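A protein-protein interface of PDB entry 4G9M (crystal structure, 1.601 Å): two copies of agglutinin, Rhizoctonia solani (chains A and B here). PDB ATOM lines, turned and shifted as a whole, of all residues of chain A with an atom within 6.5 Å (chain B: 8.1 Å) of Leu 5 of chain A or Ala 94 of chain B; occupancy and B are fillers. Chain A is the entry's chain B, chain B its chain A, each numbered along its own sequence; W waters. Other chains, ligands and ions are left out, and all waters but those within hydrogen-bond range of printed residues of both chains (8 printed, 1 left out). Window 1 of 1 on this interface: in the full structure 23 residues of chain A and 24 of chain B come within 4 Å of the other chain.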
ATOM      1  N   ILE A   3     -36.863 -20.312  -5.014  1.00  0.00           N
ATOM      2  CA  ILE A   3     -35.437 -20.501  -5.195  1.00  0.00           C
ATOM      3  C   ILE A   3     -34.761 -20.431  -3.847  1.00  0.00           C
ATOM      4  O   ILE A   3     -34.868 -19.434  -3.137  1.00  0.00           O
ATOM      5  CB  ILE A   3     -34.818 -19.421  -6.094  1.00  0.00           C
ATOM      6  CG1 ILE A   3     -35.377 -19.534  -7.513  1.00  0.00           C
ATOM      7  CG2 ILE A   3     -33.298 -19.547  -6.107  1.00  0.00           C
ATOM      8  CD1 ILE A   3     -35.001 -18.399  -8.412  1.00  0.00           C
ATOM      9  N   SER A   4     -34.058 -21.486  -3.478  1.00  0.00           N
ATOM     10  CA  SER A   4     -33.332 -21.482  -2.221  1.00  0.00           C
ATOM     11  C   SER A   4     -31.946 -22.079  -2.393  1.00  0.00           C
ATOM     12  O   SER A   4     -31.713 -22.852  -3.316  1.00  0.00           O
ATOM     13  CB  SER A   4     -34.122 -22.223  -1.138  1.00  0.00           C
ATOM     14  OG  SER A   4     -34.887 -23.278  -1.691  1.00  0.00           O
ATOM     15  N   LEU A   5     -31.039 -21.698  -1.502  1.00  0.00           N
ATOM     16  CA  LEU A   5     -29.700 -22.266  -1.457  1.00  0.00           C
ATOM     17  C   LEU A   5     -29.636 -23.062  -0.160  1.00  0.00           C
ATOM     18  O   LEU A   5     -29.349 -22.501   0.898  1.00  0.00           O
ATOM     19  CB  LEU A   5     -28.669 -21.132  -1.447  1.00  0.00           C
ATOM     20  CG  LEU A   5     -27.195 -21.504  -1.618  1.00  0.00           C
ATOM     21  CD1 LEU A   5     -26.931 -21.950  -3.062  1.00  0.00           C
ATOM     22  CD2 LEU A   5     -26.248 -20.342  -1.222  1.00  0.00           C
ATOM     23  N   PRO A   6     -29.913 -24.375  -0.220  1.00  0.00           N
ATOM     24  CA  PRO A   6     -29.986 -25.170   1.009  1.00  0.00           C
ATOM     25  C   PRO A   6     -28.606 -25.555   1.518  1.00  0.00           C
ATOM     26  O   PRO A   6     -27.634 -25.584   0.751  1.00  0.00           O
ATOM     27  CB  PRO A   6     -30.720 -26.437   0.554  1.00  0.00           C
ATOM     28  CG  PRO A   6     -30.326 -26.573  -0.893  1.00  0.00           C
ATOM     29  CD  PRO A   6     -30.281 -25.163  -1.412  1.00  0.00           C
ATOM     30  N   ALA A   7     -28.521 -25.881   2.802  1.00  0.00           N
ATOM     31  CA  ALA A   7     -27.322 -26.529   3.294  1.00  0.00           C
ATOM     32  C   ALA A   7     -27.183 -27.811   2.483  1.00  0.00           C
ATOM     33  O   ALA A   7     -28.178 -28.492   2.204  1.00  0.00           O
ATOM     34  CB  ALA A   7     -27.462 -26.854   4.784  1.00  0.00           C
ATOM     35  N   TYR A  10     -21.645 -28.723  -2.357  1.00  0.00           N
ATOM     36  CA  TYR A  10     -21.588 -27.971  -3.607  1.00  0.00           C
ATOM     37  C   TYR A  10     -20.268 -28.113  -4.361  1.00  0.00           C
ATOM     38  O   TYR A  10     -19.208 -28.294  -3.753  1.00  0.00           O
ATOM     39  CB  TYR A  10     -21.832 -26.490  -3.332  1.00  0.00           C
ATOM     40  CG  TYR A  10     -23.248 -26.143  -2.920  1.00  0.00           C
ATOM     41  CD1 TYR A  10     -23.667 -26.275  -1.599  1.00  0.00           C
ATOM     42  CD2 TYR A  10     -24.159 -25.679  -3.851  1.00  0.00           C
ATOM     43  CE1 TYR A  10     -24.974 -25.953  -1.229  1.00  0.00           C
ATOM     44  CE2 TYR A  10     -25.455 -25.359  -3.497  1.00  0.00           C
ATOM     45  CZ  TYR A  10     -25.853 -25.494  -2.190  1.00  0.00           C
ATOM     46  OH  TYR A  10     -27.139 -25.149  -1.877  1.00  0.00           O
ATOM     47  N   LEU A  49     -21.857 -26.698   2.723  1.00  0.00           N
ATOM     48  CA  LEU A  49     -22.380 -25.411   3.147  1.00  0.00           C
ATOM     49  C   LEU A  49     -23.282 -25.650   4.355  1.00  0.00           C
ATOM     50  O   LEU A  49     -24.218 -26.433   4.279  1.00  0.00           O
ATOM     51  CB  LEU A  49     -23.178 -24.761   2.003  1.00  0.00           C
ATOM     52  CG  LEU A  49     -23.915 -23.462   2.320  1.00  0.00           C
ATOM     53  CD1 LEU A  49     -22.905 -22.332   2.515  1.00  0.00           C
ATOM     54  CD2 LEU A  49     -24.898 -23.108   1.211  1.00  0.00           C
ATOM     55  N   TRP A  51     -25.086 -23.531   7.907  1.00  0.00           N
ATOM     56  CA  TRP A  51     -25.296 -22.331   8.719  1.00  0.00           C
ATOM     57  C   TRP A  51     -24.797 -22.554  10.149  1.00  0.00           C
ATOM     58  O   TRP A  51     -24.996 -23.627  10.712  1.00  0.00           O
ATOM     59  CB  TRP A  51     -26.770 -21.880   8.659  1.00  0.00           C
ATOM     60  CG  TRP A  51     -27.008 -20.991   7.479  1.00  0.00           C
ATOM     61  CD1 TRP A  51     -27.006 -19.618   7.465  1.00  0.00           C
ATOM     62  CD2 TRP A  51     -27.190 -21.403   6.120  1.00  0.00           C
ATOM     63  NE1 TRP A  51     -27.206 -19.156   6.182  1.00  0.00           N
ATOM     64  CE2 TRP A  51     -27.309 -20.231   5.337  1.00  0.00           C
ATOM     65  CE3 TRP A  51     -27.253 -22.647   5.483  1.00  0.00           C
ATOM     66  CZ2 TRP A  51     -27.498 -20.273   3.961  1.00  0.00           C
ATOM     67  CZ3 TRP A  51     -27.449 -22.686   4.111  1.00  0.00           C
ATOM     68  CH2 TRP A  51     -27.568 -21.504   3.364  1.00  0.00           C
ATOM     69  N   ASN A  56     -26.905 -14.939   9.630  1.00  0.00           N
ATOM     70  CA  ASN A  56     -26.966 -15.662   8.372  1.00  0.00           C
ATOM     71  C   ASN A  56     -25.624 -16.297   8.018  1.00  0.00           C
ATOM     72  O   ASN A  56     -25.419 -16.693   6.883  1.00  0.00           O
ATOM     73  CB  ASN A  56     -27.398 -14.749   7.220  1.00  0.00           C
ATOM     74  CG  ASN A  56     -28.676 -13.994   7.521  1.00  0.00           C
ATOM     75  OD1 ASN A  56     -28.736 -12.780   7.367  1.00  0.00           O
ATOM     76  ND2 ASN A  56     -29.698 -14.708   7.968  1.00  0.00           N
ATOM     77  N   GLN A  57     -24.719 -16.403   8.992  1.00  0.00           N
ATOM     78  CA  GLN A  57     -23.358 -16.864   8.703  1.00  0.00           C
ATOM     79  C   GLN A  57     -23.258 -18.361   8.434  1.00  0.00           C
ATOM     80  O   GLN A  57     -23.971 -19.158   9.046  1.00  0.00           O
ATOM     81  CB  GLN A  57     -22.401 -16.468   9.826  1.00  0.00           C
ATOM     82  CG  GLN A  57     -22.410 -14.979  10.077  1.00  0.00           C
ATOM     83  CD  GLN A  57     -21.442 -14.552  11.148  1.00  0.00           C
ATOM     84  OE1 GLN A  57     -20.613 -15.343  11.604  1.00  0.00           O
ATOM     85  NE2 GLN A  57     -21.528 -13.292  11.549  1.00  0.00           N
ATOM     86  N   VAL A  58     -22.358 -18.723   7.521  1.00  0.00           N
ATOM     87  CA  VAL A  58     -22.113 -20.104   7.136  1.00  0.00           C
ATOM     88  C   VAL A  58     -20.637 -20.441   7.225  1.00  0.00           C
ATOM     89  O   VAL A  58     -19.784 -19.555   7.409  1.00  0.00           O
ATOM     90  CB  VAL A  58     -22.552 -20.397   5.669  1.00  0.00           C
ATOM     91  CG1 VAL A  58     -24.009 -20.054   5.481  1.00  0.00           C
ATOM     92  CG2 VAL A  58     -21.685 -19.603   4.667  1.00  0.00           C
ATOM     93  N   ASP A  91     -20.635 -15.054   4.500  1.00  0.00           N
ATOM     94  CA  ASP A  91     -21.984 -14.661   4.105  1.00  0.00           C
ATOM     95  C   ASP A  91     -22.050 -14.931   2.613  1.00  0.00           C
ATOM     96  O   ASP A  91     -21.144 -14.535   1.876  1.00  0.00           O
ATOM     97  CB  ASP A  91     -22.193 -13.163   4.311  1.00  0.00           C
ATOM     98  CG  ASP A  91     -22.566 -12.795   5.738  1.00  0.00           C
ATOM     99  OD1 ASP A  91     -23.178 -13.633   6.458  1.00  0.00           O
ATOM    100  OD2 ASP A  91     -22.303 -11.625   6.116  1.00  0.00           O
ATOM    101  N   ILE A  92     -23.103 -15.601   2.151  1.00  0.00           N
ATOM    102  CA  ILE A  92     -23.239 -15.872   0.722  1.00  0.00           C
ATOM    103  C   ILE A  92     -24.214 -14.835   0.147  1.00  0.00           C
ATOM    104  O   ILE A  92     -25.394 -14.827   0.503  1.00  0.00           O
ATOM    105  CB  ILE A  92     -23.761 -17.308   0.470  1.00  0.00           C
ATOM    106  CG1 ILE A  92     -22.953 -18.331   1.285  1.00  0.00           C
ATOM    107  CG2 ILE A  92     -23.668 -17.649  -1.004  1.00  0.00           C
ATOM    108  CD1 ILE A  92     -21.429 -18.239   1.038  1.00  0.00           C
ATOM    109  N   VAL A  93     -23.714 -13.961  -0.723  1.00  0.00           N
ATOM    110  CA  VAL A  93     -24.469 -12.787  -1.186  1.00  0.00           C
ATOM    111  C   VAL A  93     -24.806 -12.915  -2.667  1.00  0.00           C
ATOM    112  O   VAL A  93     -23.914 -13.093  -3.492  1.00  0.00           O
ATOM    113  CB  VAL A  93     -23.638 -11.474  -0.986  1.00  0.00           C
ATOM    114  CG1 VAL A  93     -24.478 -10.264  -1.288  1.00  0.00           C
ATOM    115  CG2 VAL A  93     -23.085 -11.391   0.443  1.00  0.00           C
ATOM    116  N   ALA A  94     -26.091 -12.840  -3.012  1.00  0.00           N
ATOM    117  CA  ALA A  94     -26.500 -12.918  -4.422  1.00  0.00           C
ATOM    118  C   ALA A  94     -25.814 -11.877  -5.317  1.00  0.00           C
ATOM    119  O   ALA A  94     -25.821 -10.685  -5.023  1.00  0.00           O
ATOM    120  CB  ALA A  94     -28.020 -12.800  -4.542  1.00  0.00           C
ATOM    121  N   PHE A  99     -22.885 -16.117  -6.827  1.00  0.00           N
ATOM    122  CA  PHE A  99     -22.868 -15.527  -5.499  1.00  0.00           C
ATOM    123  C   PHE A  99     -21.465 -15.058  -5.123  1.00  0.00           C
ATOM    124  O   PHE A  99     -20.470 -15.703  -5.458  1.00  0.00           O
ATOM    125  CB  PHE A  99     -23.323 -16.569  -4.457  1.00  0.00           C
ATOM    126  CG  PHE A  99     -24.770 -17.014  -4.599  1.00  0.00           C
ATOM    127  CD1 PHE A  99     -25.122 -18.040  -5.464  1.00  0.00           C
ATOM    128  CD2 PHE A  99     -25.769 -16.386  -3.867  1.00  0.00           C
ATOM    129  CE1 PHE A  99     -26.449 -18.443  -5.592  1.00  0.00           C
ATOM    130  CE2 PHE A  99     -27.097 -16.777  -3.998  1.00  0.00           C
ATOM    131  CZ  PHE A  99     -27.432 -17.803  -4.860  1.00  0.00           C
ATOM    132  N   PHE A 139     -22.950 -21.747  -7.457  1.00  0.00           N
ATOM    133  CA  PHE A 139     -23.186 -22.774  -6.457  1.00  0.00           C
ATOM    134  C   PHE A 139     -23.903 -23.953  -7.087  1.00  0.00           C
ATOM    135  O   PHE A 139     -25.111 -23.921  -7.286  1.00  0.00           O
ATOM    136  CB  PHE A 139     -23.983 -22.205  -5.281  1.00  0.00           C
ATOM    137  CG  PHE A 139     -23.119 -21.544  -4.241  1.00  0.00           C
ATOM    138  CD1 PHE A 139     -22.360 -20.425  -4.554  1.00  0.00           C
ATOM    139  CD2 PHE A 139     -23.064 -22.048  -2.946  1.00  0.00           C
ATOM    140  CE1 PHE A 139     -21.553 -19.824  -3.607  1.00  0.00           C
ATOM    141  CE2 PHE A 139     -22.263 -21.430  -1.981  1.00  0.00           C
ATOM    142  CZ  PHE A 139     -21.514 -20.321  -2.316  1.00  0.00           C
ATOM    143  N   ASP A 141     -25.313 -27.390  -6.620  1.00  0.00           N
ATOM    144  CA  ASP A 141     -25.801 -28.315  -5.596  1.00  0.00           C
ATOM    145  C   ASP A 141     -25.720 -29.774  -6.045  1.00  0.00           C
ATOM    146  O   ASP A 141     -26.225 -30.132  -7.110  1.00  0.00           O
ATOM    147  CB  ASP A 141     -27.267 -27.955  -5.274  1.00  0.00           C
ATOM    148  CG  ASP A 141     -27.797 -28.604  -3.995  1.00  0.00           C
ATOM    149  OD1 ASP A 141     -27.015 -28.919  -3.071  1.00  0.00           O
ATOM    150  OD2 ASP A 141     -29.039 -28.742  -3.895  1.00  0.00           O
ATOM    151  N   ALA B   1     -27.850 -29.392  -9.128  1.00  0.00           N
ATOM    152  CA  ALA B   1     -28.142 -28.358 -10.111  1.00  0.00           C
ATOM    153  C   ALA B   1     -27.522 -27.007  -9.740  1.00  0.00           C
ATOM    154  O   ALA B   1     -27.367 -26.686  -8.560  1.00  0.00           O
ATOM    155  CB  ALA B   1     -29.646 -28.221 -10.285  1.00  0.00           C
ATOM    156  N   PRO B   2     -27.157 -26.209 -10.754  1.00  0.00           N
ATOM    157  CA  PRO B   2     -26.715 -24.841 -10.476  1.00  0.00           C
ATOM    158  C   PRO B   2     -27.859 -24.043  -9.857  1.00  0.00           C
ATOM    159  O   PRO B   2     -28.978 -24.051 -10.377  1.00  0.00           O
ATOM    160  CB  PRO B   2     -26.355 -24.300 -11.863  1.00  0.00           C
ATOM    161  CG  PRO B   2     -27.071 -25.170 -12.829  1.00  0.00           C
ATOM    162  CD  PRO B   2     -27.117 -26.526 -12.193  1.00  0.00           C
ATOM    163  N   ILE B   3     -27.596 -23.386  -8.736  1.00  0.00           N
ATOM    164  CA  ILE B   3     -28.629 -22.583  -8.101  1.00  0.00           C
ATOM    165  C   ILE B   3     -28.351 -21.103  -8.294  1.00  0.00           C
ATOM    166  O   ILE B   3     -27.318 -20.594  -7.866  1.00  0.00           O
ATOM    167  CB  ILE B   3     -28.758 -22.908  -6.609  1.00  0.00           C
ATOM    168  CG1 ILE B   3     -29.262 -24.348  -6.437  1.00  0.00           C
ATOM    169  CG2 ILE B   3     -29.705 -21.919  -5.938  1.00  0.00           C
ATOM    170  CD1 ILE B   3     -29.343 -24.795  -5.001  1.00  0.00           C
ATOM    171  N   SER B   4     -29.268 -20.418  -8.969  1.00  0.00           N
ATOM    172  CA  SER B   4     -29.093 -19.000  -9.248  1.00  0.00           C
ATOM    173  C   SER B   4     -30.323 -18.209  -8.854  1.00  0.00           C
ATOM    174  O   SER B   4     -31.446 -18.697  -8.946  1.00  0.00           O
ATOM    175  CB  SER B   4     -28.808 -18.769 -10.737  1.00  0.00           C
ATOM    176  OG  SER B   4     -29.811 -19.366 -11.541  1.00  0.00           O
ATOM    177  N   LEU B   5     -30.087 -16.973  -8.440  1.00  0.00           N
ATOM    178  CA  LEU B   5     -31.151 -16.018  -8.184  1.00  0.00           C
ATOM    179  C   LEU B   5     -31.076 -14.956  -9.276  1.00  0.00           C
ATOM    180  O   LEU B   5     -30.379 -13.950  -9.126  1.00  0.00           O
ATOM    181  CB  LEU B   5     -30.939 -15.379  -6.820  1.00  0.00           C
ATOM    182  CG  LEU B   5     -32.142 -14.708  -6.174  1.00  0.00           C
ATOM    183  CD1 LEU B   5     -33.198 -15.763  -5.819  1.00  0.00           C
ATOM    184  CD2 LEU B   5     -31.714 -13.938  -4.934  1.00  0.00           C
ATOM    185  N   ASP B  91     -28.695  -5.807  -0.147  1.00  0.00           N
ATOM    186  CA  ASP B  91     -27.956  -7.041  -0.399  1.00  0.00           C
ATOM    187  C   ASP B  91     -28.912  -8.189  -0.082  1.00  0.00           C
ATOM    188  O   ASP B  91     -29.597  -8.157   0.946  1.00  0.00           O
ATOM    189  CB  ASP B  91     -26.716  -7.153   0.506  1.00  0.00           C
ATOM    190  CG  ASP B  91     -25.550  -6.265   0.053  1.00  0.00           C
ATOM    191  OD1 ASP B  91     -25.268  -6.165  -1.168  1.00  0.00           O
ATOM    192  OD2 ASP B  91     -24.878  -5.700   0.940  1.00  0.00           O
ATOM    193  N   ILE B  92     -28.954  -9.202  -0.949  1.00  0.00           N
ATOM    194  CA  ILE B  92     -29.718 -10.414  -0.682  1.00  0.00           C
ATOM    195  C   ILE B  92     -28.755 -11.483  -0.183  1.00  0.00           C
ATOM    196  O   ILE B  92     -27.884 -11.948  -0.928  1.00  0.00           O
ATOM    197  CB  ILE B  92     -30.435 -10.911  -1.960  1.00  0.00           C
ATOM    198  CG1 ILE B  92     -31.142  -9.740  -2.674  1.00  0.00           C
ATOM    199  CG2 ILE B  92     -31.373 -12.043  -1.644  1.00  0.00           C
ATOM    200  CD1 ILE B  92     -32.053  -8.900  -1.789  1.00  0.00           C
ATOM    201  N   VAL B  93     -28.917 -11.875   1.077  1.00  0.00           N
ATOM    202  CA  VAL B  93     -27.956 -12.752   1.748  1.00  0.00           C
ATOM    203  C   VAL B  93     -28.608 -14.095   2.086  1.00  0.00           C
ATOM    204  O   VAL B  93     -29.678 -14.135   2.689  1.00  0.00           O
ATOM    205  CB  VAL B  93     -27.414 -12.085   3.050  1.00  0.00           C
ATOM    206  CG1 VAL B  93     -26.424 -12.992   3.754  1.00  0.00           C
ATOM    207  CG2 VAL B  93     -26.781 -10.721   2.745  1.00  0.00           C
ATOM    208  N   ALA B  94     -27.971 -15.194   1.686  1.00  0.00           N
ATOM    209  CA  ALA B  94     -28.562 -16.517   1.869  1.00  0.00           C
ATOM    210  C   ALA B  94     -28.729 -16.813   3.351  1.00  0.00           C
ATOM    211  O   ALA B  94     -27.801 -16.601   4.135  1.00  0.00           O
ATOM    212  CB  ALA B  94     -27.689 -17.583   1.205  1.00  0.00           C
ATOM    213  N   ALA B  95     -29.920 -17.276   3.728  1.00  0.00           N
ATOM    214  CA  ALA B  95     -30.161 -17.695   5.116  1.00  0.00           C
ATOM    215  C   ALA B  95     -30.513 -19.169   5.207  1.00  0.00           C
ATOM    216  O   ALA B  95     -30.727 -19.839   4.185  1.00  0.00           O
ATOM    217  CB  ALA B  95     -31.257 -16.835   5.771  1.00  0.00           C
ATOM    218  N   ASP B  96     -30.573 -19.680   6.434  1.00  0.00           N
ATOM    219  CA  ASP B  96     -30.910 -21.085   6.659  1.00  0.00           C
ATOM    220  C   ASP B  96     -32.301 -21.415   6.122  1.00  0.00           C
ATOM    221  O   ASP B  96     -32.572 -22.557   5.778  1.00  0.00           O
ATOM    222  CB  ASP B  96     -30.787 -21.456   8.142  1.00  0.00           C
ATOM    223  CG  ASP B  96     -31.845 -20.796   9.002  1.00  0.00           C
ATOM    224  OD1 ASP B  96     -31.861 -19.554   9.061  1.00  0.00           O
ATOM    225  OD2 ASP B  96     -32.651 -21.524   9.638  1.00  0.00           O
ATOM    226  N   LYS B  97     -33.172 -20.407   6.083  1.00  0.00           N
ATOM    227  CA  LYS B  97     -34.462 -20.465   5.392  1.00  0.00           C
ATOM    228  C   LYS B  97     -34.555 -19.201   4.550  1.00  0.00           C
ATOM    229  O   LYS B  97     -34.419 -18.092   5.076  1.00  0.00           O
ATOM    230  CB  LYS B  97     -35.620 -20.502   6.393  1.00  0.00           C
ATOM    231  CG  LYS B  97     -35.660 -21.767   7.240  1.00  0.00           C
ATOM    232  CD  LYS B  97     -36.729 -21.686   8.306  1.00  0.00           C
ATOM    233  CE  LYS B  97     -36.660 -22.890   9.250  1.00  0.00           C
ATOM    234  NZ  LYS B  97     -37.635 -22.713  10.364  1.00  0.00           N
ATOM    235  N   GLY B  98     -34.757 -19.350   3.245  1.00  0.00           N
ATOM    236  CA  GLY B  98     -34.897 -18.188   2.383  1.00  0.00           C
ATOM    237  C   GLY B  98     -33.663 -17.286   2.339  1.00  0.00           C
ATOM    238  O   GLY B  98     -32.522 -17.756   2.413  1.00  0.00           O
ATOM    239  N   PHE B  99     -33.910 -15.992   2.203  1.00  0.00           N
ATOM    240  CA  PHE B  99     -32.860 -14.976   2.156  1.00  0.00           C
ATOM    241  C   PHE B  99     -33.162 -13.821   3.095  1.00  0.00           C
ATOM    242  O   PHE B  99     -34.313 -13.425   3.275  1.00  0.00           O
ATOM    243  CB  PHE B  99     -32.708 -14.406   0.739  1.00  0.00           C
ATOM    244  CG  PHE B  99     -32.203 -15.406  -0.275  1.00  0.00           C
ATOM    245  CD1 PHE B  99     -30.850 -15.501  -0.566  1.00  0.00           C
ATOM    246  CD2 PHE B  99     -33.091 -16.227  -0.952  1.00  0.00           C
ATOM    247  CE1 PHE B  99     -30.383 -16.412  -1.505  1.00  0.00           C
ATOM    248  CE2 PHE B  99     -32.634 -17.152  -1.889  1.00  0.00           C
ATOM    249  CZ  PHE B  99     -31.285 -17.246  -2.166  1.00  0.00           C
ATOM    250  N   ALA B 100     -32.111 -13.245   3.664  1.00  0.00           N
ATOM    251  CA  ALA B 100     -32.233 -11.957   4.332  1.00  0.00           C
ATOM    252  C   ALA B 100     -32.053 -10.842   3.301  1.00  0.00           C
ATOM    253  O   ALA B 100     -31.281 -10.967   2.358  1.00  0.00           O
ATOM    254  CB  ALA B 100     -31.203 -11.823   5.443  1.00  0.00           C
ATOM    255  N   ILE B 101     -32.793  -9.762   3.479  1.00  0.00           N
ATOM    256  CA  ILE B 101     -32.683  -8.604   2.602  1.00  0.00           C
ATOM    257  C   ILE B 101     -32.115  -7.477   3.440  1.00  0.00           C
ATOM    258  O   ILE B 101     -32.821  -6.898   4.261  1.00  0.00           O
ATOM    259  CB  ILE B 101     -34.065  -8.234   2.042  1.00  0.00           C
ATOM    260  CG1 ILE B 101     -34.709  -9.475   1.391  1.00  0.00           C
ATOM    261  CG2 ILE B 101     -33.969  -7.025   1.080  1.00  0.00           C
ATOM    262  CD1 ILE B 101     -36.119  -9.231   0.861  1.00  0.00           C
ATOM    263  N   GLU B 102     -30.830  -7.184   3.233  1.00  0.00           N
ATOM    264  CA  GLU B 102     -30.074  -6.231   4.049  1.00  0.00           C
ATOM    265  C   GLU B 102     -30.017  -4.851   3.425  1.00  0.00           C
ATOM    266  O   GLU B 102     -29.965  -4.720   2.203  1.00  0.00           O
ATOM    267  CB  GLU B 102     -28.621  -6.697   4.186  1.00  0.00           C
ATOM    268  CG  GLU B 102     -28.350  -7.732   5.234  1.00  0.00           C
ATOM    269  CD  GLU B 102     -26.866  -8.037   5.376  1.00  0.00           C
ATOM    270  OE1 GLU B 102     -26.066  -7.557   4.543  1.00  0.00           O
ATOM    271  OE2 GLU B 102     -26.502  -8.763   6.320  1.00  0.00           O
ATOM    272  N   ASN B 129     -30.529  -7.316  12.455  1.00  0.00           N
ATOM    273  CA  ASN B 129     -30.565  -8.713  12.008  1.00  0.00           C
ATOM    274  C   ASN B 129     -30.245  -9.728  13.111  1.00  0.00           C
ATOM    275  O   ASN B 129     -29.100  -9.849  13.544  1.00  0.00           O
ATOM    276  CB  ASN B 129     -29.623  -8.913  10.818  1.00  0.00           C
ATOM    277  CG  ASN B 129     -29.837 -10.242  10.113  1.00  0.00           C
ATOM    278  OD1 ASN B 129     -30.799 -10.967  10.396  1.00  0.00           O
ATOM    279  ND2 ASN B 129     -28.936 -10.572   9.196  1.00  0.00           N
ATOM    280  N   LYS B 136     -36.505 -13.311   7.301  1.00  0.00           N
ATOM    281  CA  LYS B 136     -36.080 -14.137   6.169  1.00  0.00           C
ATOM    282  C   LYS B 136     -37.220 -14.221   5.161  1.00  0.00           C
ATOM    283  O   LYS B 136     -38.383 -14.258   5.546  1.00  0.00           O
ATOM    284  CB  LYS B 136     -35.701 -15.544   6.650  1.00  0.00           C
ATOM    285  CG  LYS B 136     -34.536 -15.547   7.634  1.00  0.00           C
ATOM    286  CD  LYS B 136     -34.363 -16.911   8.293  1.00  0.00           C
ATOM    287  CE  LYS B 136     -33.602 -16.813   9.596  1.00  0.00           C
ATOM    288  NZ  LYS B 136     -33.648 -18.095  10.381  1.00  0.00           N
ATOM    289  N   TRP B 137     -36.879 -14.257   3.877  1.00  0.00           N
ATOM    290  CA  TRP B 137     -37.870 -14.134   2.809  1.00  0.00           C
ATOM    291  C   TRP B 137     -37.632 -15.183   1.731  1.00  0.00           C
ATOM    292  O   TRP B 137     -36.503 -15.355   1.266  1.00  0.00           O
ATOM    293  CB  TRP B 137     -37.827 -12.723   2.197  1.00  0.00           C
ATOM    294  CG  TRP B 137     -38.120 -11.628   3.186  1.00  0.00           C
ATOM    295  CD1 TRP B 137     -37.226 -11.002   4.008  1.00  0.00           C
ATOM    296  CD2 TRP B 137     -39.403 -11.050   3.471  1.00  0.00           C
ATOM    297  NE1 TRP B 137     -37.872 -10.067   4.780  1.00  0.00           N
ATOM    298  CE2 TRP B 137     -39.208 -10.077   4.471  1.00  0.00           C
ATOM    299  CE3 TRP B 137     -40.697 -11.262   2.975  1.00  0.00           C
ATOM    300  CZ2 TRP B 137     -40.258  -9.306   4.980  1.00  0.00           C
ATOM    301  CZ3 TRP B 137     -41.746 -10.491   3.481  1.00  0.00           C
ATOM    302  CH2 TRP B 137     -41.515  -9.528   4.478  1.00  0.00           C
HETATM  303  O   HOH W   1     -29.820 -17.546   8.991  1.00  0.00           O
HETATM  304  O   HOH W   2     -26.393 -11.144   6.959  1.00  0.00           O
HETATM  305  O   HOH W   3     -27.292  -8.954  -3.299  1.00  0.00           O
HETATM  306  O   HOH W   4     -32.133 -12.942   8.760  1.00  0.00           O
HETATM  307  O   HOH W   5     -25.041 -16.381   4.012  1.00  0.00           O
HETATM  308  O   HOH W   6     -30.521 -25.018   4.739  1.00  0.00           O
HETATM  309  O   HOH W   7     -32.345 -19.882   0.502  1.00  0.00           O
HETATM  310  O   HOH W   8     -24.924 -19.956  -8.808  1.00  0.00           O
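Of chain B, only Ile 3 comes within 4 Å of Pro 6 of chain A. Of the printed residues of chain B, Ala 94 of chain A touches Leu 5 and Ile 92. Of the printed residues of chain A, Leu 5 of chain B touches Ile 3 and Ala 94. Ala 94 of chain B touches four residues of chain A. Printed residues of chain A within 4 Å of Phe 99 of chain B: Ile 3. The nearest printed residue of chain B that does not touch Leu 5 of chain A is Ala 95 of chain B (4.4 Å). The nearest printed residue of chain B that does not touch Asp 141 of chain A is Pro 2 of chain B (4.7 Å).
Water W3 bridges O of Ala 94 of chain A (2.9 Å) and N of Ile 92 of chain B (2.9 Å).
The side-chain carboxylate (OD1) of Asp 96 of chain B lies within salt-bridge range of the side-chain amino group (NZ) of Lys 136 of chain B, 2.7 Å away.
Hydrophobic or aromatic side chains of chain B within 4 Å of the printed part of chain A: Ile 3, Leu 5, Val 93, Ala 94, Ala 95, Phe 99 and Ala 100.
Leu 5 of chain A touches Ala 94 of chain B, and with the chains exchanged Ala 94 of chain A touches Leu 5 of chain B. Ile 92 of chain A touches Val 93 of chain B, and with the chains exchanged Val 93 of chain A touches Ile 92 of chain B.
The side-chain amide nitrogen (ND2) of Asn 129 of chain B sits at hydrogen-bond distance from the side-chain amide oxygen (OD1) of Asn 56 of chain A, at 2.9 Å. The backbone NH (N) of Ile 3 of chain B lies within hydrogen-bond range of the backbone carbonyl oxygen (O) of Phe 139 of chain A, 2.9 Å away. O of Ala 94 of chain B is in hydrogen-bond range of NE1 of Trp 51 of chain A (3.3 Å). The indole nitrogen (NE1) of Trp 51 of chain A lies close to the backbone NH (N) of Asp 96 of chain B (3.4 Å). N of Ala 94 of chain B is in hydrogen-bond range of O of Ile 92 of chain A. O of Ile 92 of chain B is in hydrogen-bond range of N of Ala 94 of chain A (2.9 Å). The backbone NH of Ala 1 of chain B lies within hydrogen-bond range of the backbone carbonyl oxygen of Asp 141 of chain A, 2.7 Å away.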
